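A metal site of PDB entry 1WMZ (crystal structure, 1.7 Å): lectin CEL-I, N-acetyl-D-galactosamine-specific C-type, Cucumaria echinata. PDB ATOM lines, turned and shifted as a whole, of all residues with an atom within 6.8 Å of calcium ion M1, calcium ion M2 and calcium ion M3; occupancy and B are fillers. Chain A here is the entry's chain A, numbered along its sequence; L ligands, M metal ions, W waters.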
ATOM      1  N   ASP A  77      27.467  -0.607 -22.715  1.00  0.00           N
ATOM      2  CA  ASP A  77      28.777  -0.820 -23.324  1.00  0.00           C
ATOM      3  C   ASP A  77      29.889  -0.178 -22.473  1.00  0.00           C
ATOM      4  O   ASP A  77      30.932   0.229 -22.997  1.00  0.00           O
ATOM      5  CB  ASP A  77      28.795  -0.309 -24.770  1.00  0.00           C
ATOM      6  CG  ASP A  77      29.012   1.183 -24.869  1.00  0.00           C
ATOM      7  OD1 ASP A  77      28.596   1.933 -23.953  1.00  0.00           O
ATOM      8  OD2 ASP A  77      29.620   1.701 -25.843  1.00  0.00           O
ATOM      9  N   LYS A  78      29.666  -0.107 -21.161  1.00  0.00           N
ATOM     10  CA  LYS A  78      30.632   0.441 -20.190  1.00  0.00           C
ATOM     11  C   LYS A  78      31.976  -0.285 -20.229  1.00  0.00           C
ATOM     12  O   LYS A  78      33.040   0.363 -20.187  1.00  0.00           O
ATOM     13  CB  LYS A  78      30.072   0.332 -18.766  1.00  0.00           C
ATOM     14  CG  LYS A  78      30.952   0.969 -17.688  1.00  0.00           C
ATOM     15  CD  LYS A  78      30.874   0.166 -16.410  1.00  0.00           C
ATOM     16  CE  LYS A  78      31.642   0.810 -15.252  1.00  0.00           C
ATOM     17  NZ  LYS A  78      30.756   1.636 -14.340  1.00  0.00           N
ATOM     18  N   TYR A  79      31.926  -1.618 -20.278  1.00  0.00           N
ATOM     19  CA  TYR A  79      33.120  -2.448 -20.163  1.00  0.00           C
ATOM     20  C   TYR A  79      33.939  -2.445 -21.450  1.00  0.00           C
ATOM     21  O   TYR A  79      35.160  -2.377 -21.391  1.00  0.00           O
ATOM     22  CB  TYR A  79      32.754  -3.883 -19.722  1.00  0.00           C
ATOM     23  CG  TYR A  79      32.449  -3.979 -18.228  1.00  0.00           C
ATOM     24  CD1 TYR A  79      31.140  -4.080 -17.764  1.00  0.00           C
ATOM     25  CD2 TYR A  79      33.484  -3.973 -17.268  1.00  0.00           C
ATOM     26  CE1 TYR A  79      30.859  -4.163 -16.394  1.00  0.00           C
ATOM     27  CE2 TYR A  79      33.204  -4.054 -15.888  1.00  0.00           C
ATOM     28  CZ  TYR A  79      31.892  -4.155 -15.466  1.00  0.00           C
ATOM     29  OH  TYR A  79      31.589  -4.230 -14.114  1.00  0.00           O
ATOM     30  N   ASN A  80      33.282  -2.505 -22.620  1.00  0.00           N
ATOM     31  CA  ASN A  80      33.950  -2.396 -23.944  1.00  0.00           C
ATOM     32  C   ASN A  80      33.190  -1.450 -24.896  1.00  0.00           C
ATOM     33  O   ASN A  80      32.168  -1.833 -25.508  1.00  0.00           O
ATOM     34  CB  ASN A  80      34.085  -3.771 -24.630  1.00  0.00           C
ATOM     35  CG  ASN A  80      35.103  -4.691 -23.937  1.00  0.00           C
ATOM     36  OD1 ASN A  80      36.297  -4.459 -24.000  1.00  0.00           O
ATOM     37  ND2 ASN A  80      34.602  -5.761 -23.297  1.00  0.00           N
ATOM     38  N   GLU A  81      33.704  -0.224 -25.036  1.00  0.00           N
ATOM     39  CA  GLU A  81      33.067   0.806 -25.878  1.00  0.00           C
ATOM     40  C   GLU A  81      32.674   0.288 -27.250  1.00  0.00           C
ATOM     41  O   GLU A  81      33.500  -0.288 -27.989  1.00  0.00           O
ATOM     42  CB  GLU A  81      33.971   2.032 -26.000  1.00  0.00           C
ATOM     43  CG  GLU A  81      33.349   3.211 -26.793  1.00  0.00           C
ATOM     44  CD  GLU A  81      31.984   3.681 -26.286  1.00  0.00           C
ATOM     45  OE1 GLU A  81      31.103   3.965 -27.112  1.00  0.00           O
ATOM     46  OE2 GLU A  81      31.805   3.789 -25.065  1.00  0.00           O
ATOM     47  N   GLY A  82      31.390   0.487 -27.569  1.00  0.00           N
ATOM     48  CA  GLY A  82      30.774   0.074 -28.812  1.00  0.00           C
ATOM     49  C   GLY A  82      30.174  -1.309 -28.871  1.00  0.00           C
ATOM     50  O   GLY A  82      29.426  -1.606 -29.789  1.00  0.00           O
ATOM     51  N   PHE A  84      27.651  -3.427 -27.172  1.00  0.00           N
ATOM     52  CA  PHE A  84      26.503  -3.404 -26.259  1.00  0.00           C
ATOM     53  C   PHE A  84      26.122  -4.819 -25.861  1.00  0.00           C
ATOM     54  O   PHE A  84      26.063  -5.725 -26.721  1.00  0.00           O
ATOM     55  CB  PHE A  84      25.343  -2.617 -26.857  1.00  0.00           C
ATOM     56  CG  PHE A  84      25.522  -1.126 -26.695  1.00  0.00           C
ATOM     57  CD1 PHE A  84      25.099  -0.498 -25.542  1.00  0.00           C
ATOM     58  CD2 PHE A  84      26.149  -0.377 -27.700  1.00  0.00           C
ATOM     59  CE1 PHE A  84      25.246   0.846 -25.352  1.00  0.00           C
ATOM     60  CE2 PHE A  84      26.315   0.997 -27.532  1.00  0.00           C
ATOM     61  CZ  PHE A  84      25.878   1.619 -26.353  1.00  0.00           C
ATOM     62  N   GLY A 100      20.438   7.322 -35.927  1.00  0.00           N
ATOM     63  CA  GLY A 100      21.579   8.097 -35.416  1.00  0.00           C
ATOM     64  C   GLY A 100      22.186   7.586 -34.116  1.00  0.00           C
ATOM     65  O   GLY A 100      23.139   8.192 -33.586  1.00  0.00           O
ATOM     66  N   GLN A 101      21.634   6.468 -33.632  1.00  0.00           N
ATOM     67  CA  GLN A 101      22.047   5.854 -32.357  1.00  0.00           C
ATOM     68  C   GLN A 101      22.511   4.408 -32.584  1.00  0.00           C
ATOM     69  O   GLN A 101      22.032   3.736 -33.514  1.00  0.00           O
ATOM     70  CB  GLN A 101      20.844   5.846 -31.392  1.00  0.00           C
ATOM     71  CG  GLN A 101      20.229   7.218 -31.133  1.00  0.00           C
ATOM     72  CD  GLN A 101      21.190   8.228 -30.541  1.00  0.00           C
ATOM     73  OE1 GLN A 101      22.198   7.879 -29.985  1.00  0.00           O
ATOM     74  NE2 GLN A 101      20.883   9.513 -30.709  1.00  0.00           N
ATOM     75  N   PRO A 102      23.414   3.903 -31.759  1.00  0.00           N
ATOM     76  CA  PRO A 102      24.063   4.614 -30.649  1.00  0.00           C
ATOM     77  C   PRO A 102      25.192   5.503 -31.167  1.00  0.00           C
ATOM     78  O   PRO A 102      25.767   5.217 -32.219  1.00  0.00           O
ATOM     79  CB  PRO A 102      24.668   3.459 -29.826  1.00  0.00           C
ATOM     80  CG  PRO A 102      25.031   2.465 -30.836  1.00  0.00           C
ATOM     81  CD  PRO A 102      23.960   2.540 -31.888  1.00  0.00           C
ATOM     82  N   ASP A 103      25.513   6.543 -30.443  1.00  0.00           N
ATOM     83  CA  ASP A 103      26.483   7.565 -30.907  1.00  0.00           C
ATOM     84  C   ASP A 103      27.541   7.947 -29.894  1.00  0.00           C
ATOM     85  O   ASP A 103      28.375   8.779 -30.169  1.00  0.00           O
ATOM     86  CB  ASP A 103      25.740   8.817 -31.432  1.00  0.00           C
ATOM     87  CG  ASP A 103      24.984   9.542 -30.342  1.00  0.00           C
ATOM     88  OD1 ASP A 103      24.467  10.690 -30.586  1.00  0.00           O
ATOM     89  OD2 ASP A 103      24.836   9.047 -29.193  1.00  0.00           O
ATOM     90  N   ASN A 104      27.536   7.353 -28.708  1.00  0.00           N
ATOM     91  CA  ASN A 104      28.485   7.685 -27.658  1.00  0.00           C
ATOM     92  C   ASN A 104      28.718   9.200 -27.504  1.00  0.00           C
ATOM     93  O   ASN A 104      29.845   9.657 -27.407  1.00  0.00           O
ATOM     94  CB  ASN A 104      29.815   6.951 -27.912  1.00  0.00           C
ATOM     95  CG  ASN A 104      30.669   6.846 -26.674  1.00  0.00           C
ATOM     96  OD1 ASN A 104      30.208   6.475 -25.579  1.00  0.00           O
ATOM     97  ND2 ASN A 104      31.945   7.134 -26.842  1.00  0.00           N
ATOM     98  N   TRP A 105      27.631   9.954 -27.483  1.00  0.00           N
ATOM     99  CA  TRP A 105      27.726  11.401 -27.458  1.00  0.00           C
ATOM    100  C   TRP A 105      28.590  11.874 -26.300  1.00  0.00           C
ATOM    101  O   TRP A 105      28.457  11.416 -25.163  1.00  0.00           O
ATOM    102  CB  TRP A 105      26.316  11.965 -27.359  1.00  0.00           C
ATOM    103  CG  TRP A 105      26.207  13.425 -27.476  1.00  0.00           C
ATOM    104  CD1 TRP A 105      26.356  14.167 -28.581  1.00  0.00           C
ATOM    105  CD2 TRP A 105      25.831  14.328 -26.423  1.00  0.00           C
ATOM    106  NE1 TRP A 105      26.090  15.487 -28.315  1.00  0.00           N
ATOM    107  CE2 TRP A 105      25.799  15.614 -26.985  1.00  0.00           C
ATOM    108  CE3 TRP A 105      25.554  14.186 -25.063  1.00  0.00           C
ATOM    109  CZ2 TRP A 105      25.478  16.747 -26.235  1.00  0.00           C
ATOM    110  CZ3 TRP A 105      25.235  15.306 -24.311  1.00  0.00           C
ATOM    111  CH2 TRP A 105      25.218  16.581 -24.906  1.00  0.00           C
ATOM    112  N   ASN A 107      31.432  11.158 -25.685  1.00  0.00           N
ATOM    113  CA  ASN A 107      32.210  10.006 -25.168  1.00  0.00           C
ATOM    114  C   ASN A 107      31.775   9.501 -23.809  1.00  0.00           C
ATOM    115  O   ASN A 107      32.555   8.896 -23.101  1.00  0.00           O
ATOM    116  CB  ASN A 107      33.689  10.371 -25.130  1.00  0.00           C
ATOM    117  CG  ASN A 107      34.212  10.806 -26.475  1.00  0.00           C
ATOM    118  OD1 ASN A 107      34.175  10.029 -27.462  1.00  0.00           O
ATOM    119  ND2 ASN A 107      34.722  12.034 -26.552  1.00  0.00           N
ATOM    120  N   ALA A 108      30.516   9.682 -23.459  1.00  0.00           N
ATOM    121  CA  ALA A 108      30.050   9.373 -22.112  1.00  0.00           C
ATOM    122  C   ALA A 108      28.712   8.616 -22.073  1.00  0.00           C
ATOM    123  O   ALA A 108      28.097   8.477 -20.997  1.00  0.00           O
ATOM    124  CB  ALA A 108      29.975  10.625 -21.300  1.00  0.00           C
ATOM    125  N   GLU A 109      28.253   8.115 -23.221  1.00  0.00           N
ATOM    126  CA  GLU A 109      26.994   7.409 -23.276  1.00  0.00           C
ATOM    127  C   GLU A 109      27.203   5.884 -23.444  1.00  0.00           C
ATOM    128  O   GLU A 109      27.563   5.400 -24.538  1.00  0.00           O
ATOM    129  CB  GLU A 109      26.073   7.960 -24.379  1.00  0.00           C
ATOM    130  CG  GLU A 109      25.843   9.467 -24.297  1.00  0.00           C
ATOM    131  CD  GLU A 109      24.721   9.919 -25.161  1.00  0.00           C
ATOM    132  OE1 GLU A 109      24.566   9.404 -26.288  1.00  0.00           O
ATOM    133  OE2 GLU A 109      23.935  10.823 -24.731  1.00  0.00           O
ATOM    134  N   ASP A 110      26.926   5.159 -22.363  1.00  0.00           N
ATOM    135  CA  ASP A 110      27.115   3.692 -22.286  1.00  0.00           C
ATOM    136  C   ASP A 110      25.892   2.898 -21.795  1.00  0.00           C
ATOM    137  O   ASP A 110      26.005   1.709 -21.535  1.00  0.00           O
ATOM    138  CB  ASP A 110      28.256   3.373 -21.338  1.00  0.00           C
ATOM    139  CG  ASP A 110      29.498   4.242 -21.565  1.00  0.00           C
ATOM    140  OD1 ASP A 110      30.078   4.670 -20.547  1.00  0.00           O
ATOM    141  OD2 ASP A 110      29.974   4.553 -22.684  1.00  0.00           O
ATOM    142  N   TYR A 111      24.757   3.540 -21.655  1.00  0.00           N
ATOM    143  CA  TYR A 111      23.595   2.970 -20.973  1.00  0.00           C
ATOM    144  C   TYR A 111      22.352   3.094 -21.844  1.00  0.00           C
ATOM    145  O   TYR A 111      21.927   4.184 -22.237  1.00  0.00           O
ATOM    146  CB  TYR A 111      23.442   3.715 -19.617  1.00  0.00           C
ATOM    147  CG  TYR A 111      24.729   3.714 -18.845  1.00  0.00           C
ATOM    148  CD1 TYR A 111      25.513   4.879 -18.714  1.00  0.00           C
ATOM    149  CD2 TYR A 111      25.224   2.533 -18.325  1.00  0.00           C
ATOM    150  CE1 TYR A 111      26.725   4.852 -18.013  1.00  0.00           C
ATOM    151  CE2 TYR A 111      26.412   2.493 -17.636  1.00  0.00           C
ATOM    152  CZ  TYR A 111      27.173   3.659 -17.479  1.00  0.00           C
ATOM    153  OH  TYR A 111      28.375   3.593 -16.830  1.00  0.00           O
ATOM    154  N   GLN A 113      18.390   2.715 -23.268  1.00  0.00           N
ATOM    155  CA  GLN A 113      17.075   3.177 -22.824  1.00  0.00           C
ATOM    156  C   GLN A 113      16.135   3.295 -24.022  1.00  0.00           C
ATOM    157  O   GLN A 113      16.574   3.591 -25.150  1.00  0.00           O
ATOM    158  CB  GLN A 113      17.198   4.524 -22.103  1.00  0.00           C
ATOM    159  CG  GLN A 113      17.808   5.640 -23.022  1.00  0.00           C
ATOM    160  CD  GLN A 113      17.861   7.093 -22.421  1.00  0.00           C
ATOM    161  OE1 GLN A 113      17.996   8.060 -23.201  1.00  0.00           O
ATOM    162  NE2 GLN A 113      17.824   7.227 -21.105  1.00  0.00           N
ATOM    163  N   ARG A 115      13.358   5.449 -25.897  1.00  0.00           N
ATOM    164  CA  ARG A 115      12.603   6.686 -26.048  1.00  0.00           C
ATOM    165  C   ARG A 115      11.100   6.476 -25.861  1.00  0.00           C
ATOM    166  O   ARG A 115      10.596   5.352 -26.007  1.00  0.00           O
ATOM    167  CB  ARG A 115      12.837   7.275 -27.427  1.00  0.00           C
ATOM    168  CG  ARG A 115      14.189   7.804 -27.632  1.00  0.00           C
ATOM    169  CD  ARG A 115      14.404   8.286 -29.026  1.00  0.00           C
ATOM    170  NE  ARG A 115      15.684   8.978 -29.173  1.00  0.00           N
ATOM    171  CZ  ARG A 115      16.173   9.363 -30.342  1.00  0.00           C
ATOM    172  NH1 ARG A 115      15.494   9.118 -31.468  1.00  0.00           N
ATOM    173  NH2 ARG A 115      17.355   9.929 -30.397  1.00  0.00           N
ATOM    174  N   ASN A 123      18.156   4.439 -27.413  1.00  0.00           N
ATOM    175  CA  ASN A 123      19.204   5.446 -27.336  1.00  0.00           C
ATOM    176  C   ASN A 123      20.229   5.026 -26.297  1.00  0.00           C
ATOM    177  O   ASN A 123      19.905   4.429 -25.272  1.00  0.00           O
ATOM    178  CB  ASN A 123      18.631   6.787 -26.913  1.00  0.00           C
ATOM    179  CG  ASN A 123      19.701   7.802 -26.675  1.00  0.00           C
ATOM    180  OD1 ASN A 123      20.517   8.055 -27.583  1.00  0.00           O
ATOM    181  ND2 ASN A 123      19.718   8.427 -25.484  1.00  0.00           N
ATOM    182  N   ASP A 124      21.495   5.359 -26.535  1.00  0.00           N
ATOM    183  CA  ASP A 124      22.472   5.292 -25.472  1.00  0.00           C
ATOM    184  C   ASP A 124      22.591   6.618 -24.777  1.00  0.00           C
ATOM    185  O   ASP A 124      22.659   7.649 -25.449  1.00  0.00           O
ATOM    186  CB  ASP A 124      23.854   4.828 -25.995  1.00  0.00           C
ATOM    187  CG  ASP A 124      24.408   5.725 -27.086  1.00  0.00           C
ATOM    188  OD1 ASP A 124      23.620   6.402 -27.786  1.00  0.00           O
ATOM    189  OD2 ASP A 124      25.630   5.751 -27.334  1.00  0.00           O
ATOM    190  N   ASN A 125      22.627   6.630 -23.443  1.00  0.00           N
ATOM    191  CA  ASN A 125      22.736   7.847 -22.649  1.00  0.00           C
ATOM    192  C   ASN A 125      23.790   7.689 -21.513  1.00  0.00           C
ATOM    193  O   ASN A 125      24.389   6.628 -21.360  1.00  0.00           O
ATOM    194  CB  ASN A 125      21.331   8.213 -22.122  1.00  0.00           C
ATOM    195  CG  ASN A 125      21.103   9.718 -22.007  1.00  0.00           C
ATOM    196  OD1 ASN A 125      22.009  10.461 -21.610  1.00  0.00           O
ATOM    197  ND2 ASN A 125      19.913  10.137 -22.280  1.00  0.00           N
HETATM  198  C1  LIG L   1      19.510  12.672 -28.507  1.00  0.00           C
HETATM  199  C2  LIG L   1      19.913  11.647 -27.418  1.00  0.00           C
HETATM  200  C3  LIG L   1      21.311  11.654 -26.854  1.00  0.00           C
HETATM  201  C4  LIG L   1      22.346  12.172 -27.808  1.00  0.00           C
HETATM  202  C5  LIG L   1      21.920  13.205 -28.819  1.00  0.00           C
HETATM  203  C6  LIG L   1      22.960  13.481 -29.925  1.00  0.00           C
HETATM  204  C7  LIG L   1      17.876  10.742 -26.448  1.00  0.00           C
HETATM  205  C8  LIG L   1      16.970  10.767 -25.249  1.00  0.00           C
HETATM  206  N1  LIG L   1      18.946  11.543 -26.366  1.00  0.00           N
HETATM  207  O1  LIG L   1      18.381  12.319 -29.308  1.00  0.00           O
HETATM  208  O2  LIG L   1      21.766  10.469 -26.187  1.00  0.00           O
HETATM  209  O3  LIG L   1      22.582  11.037 -28.652  1.00  0.00           O
HETATM  210  O4  LIG L   1      20.602  13.148 -29.330  1.00  0.00           O
HETATM  211  O5  LIG L   1      22.521  14.711 -30.511  1.00  0.00           O
HETATM  212  O6  LIG L   1      17.660  10.024 -27.413  1.00  0.00           O
HETATM  213 CA    CA M   1      29.393   4.032 -25.217  1.00  0.00          CA
HETATM  214 CA    CA M   2      22.925   8.738 -27.643  1.00  0.00          CA
HETATM  215 CA    CA M   3      32.348   4.199 -22.594  1.00  0.00          CA
HETATM  216  O   HOH W   1      32.874   2.036 -22.699  1.00  0.00           O
HETATM  217  O   HOH W   2      27.909   4.326 -27.062  1.00  0.00           O
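Of the 23 residues printed, 5 come within 4 Å of calcium ion M1.
Within 4 Å of calcium ion M3: Glu 81 and Asp 110. The nearest printed residue that does not touch calcium ion M3 is Asp 77 (4.2 Å).
Calcium ion M1 is bound by O of Glu 109 (2.4 Å), water W2 (2.4 Å), OD2 of Asp 77 (2.4 Å), OE2 of Glu 81 (2.4 Å), OE1 of Glu 81 (2.6 Å), OD1 of Asp 77 (2.6 Å), OD1 of Asn 104 (2.6 Å) and OD2 of Asp 110 (2.7 Å). Calcium ion M1 has eight donor atoms within binding distance.
Calcium ion M2 is bound by OE1 of Glu 109 (2.2 Å), OD1 of Asp 124 (2.4 Å), O of Asp 124 (2.5 Å), OD2 of Asp 103 (2.5 Å), OD1 of Asn 123 (2.5 Å), O3 of the ligand (2.5 Å), O2 of the ligand (2.5 Å) and OE1 of Gln 101 (2.6 Å).
Water W1 binds calcium ion M3. Calcium ion M3 is bound by the side-chain carboxylate (OD2) of Asp 110 (2.4 Å). OE2 of Glu 81 is bound to calcium ion M3. Slightly farther from calcium ion M3 lies OD1 of Asp 110 (3.1 Å).
N of Trp 105 lies close to OE1 of Glu 109 (3.3 Å). The backbone carbonyl oxygen of Asn 125 lies within hydrogen-bond range of the backbone NH of Asp 110 (3.1 Å). OD2 of Asp 77 sits close to N of Gly 82 (2.8 Å). OD2 of Asp 124 lies within hydrogen-bond range of N of Asn 104. The side-chain carboxylate (OD2) of Asp 103 lies close to the backbone NH (N) of Trp 105, 3.4 Å away. ND2 of Asn 123 sits at hydrogen-bond distance from OE1 of Gln 113 (2.9 Å).
The guanidinium group (NH2) of Arg 115 sits at hydrogen-bond distance from an oxygen (O1) of the ligand, at 2.8 Å.
Water W2 bridges the side-chain carboxylate of Asp 124 (2.7 Å) and the backbone NH of Asn 104 (3.5 Å).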
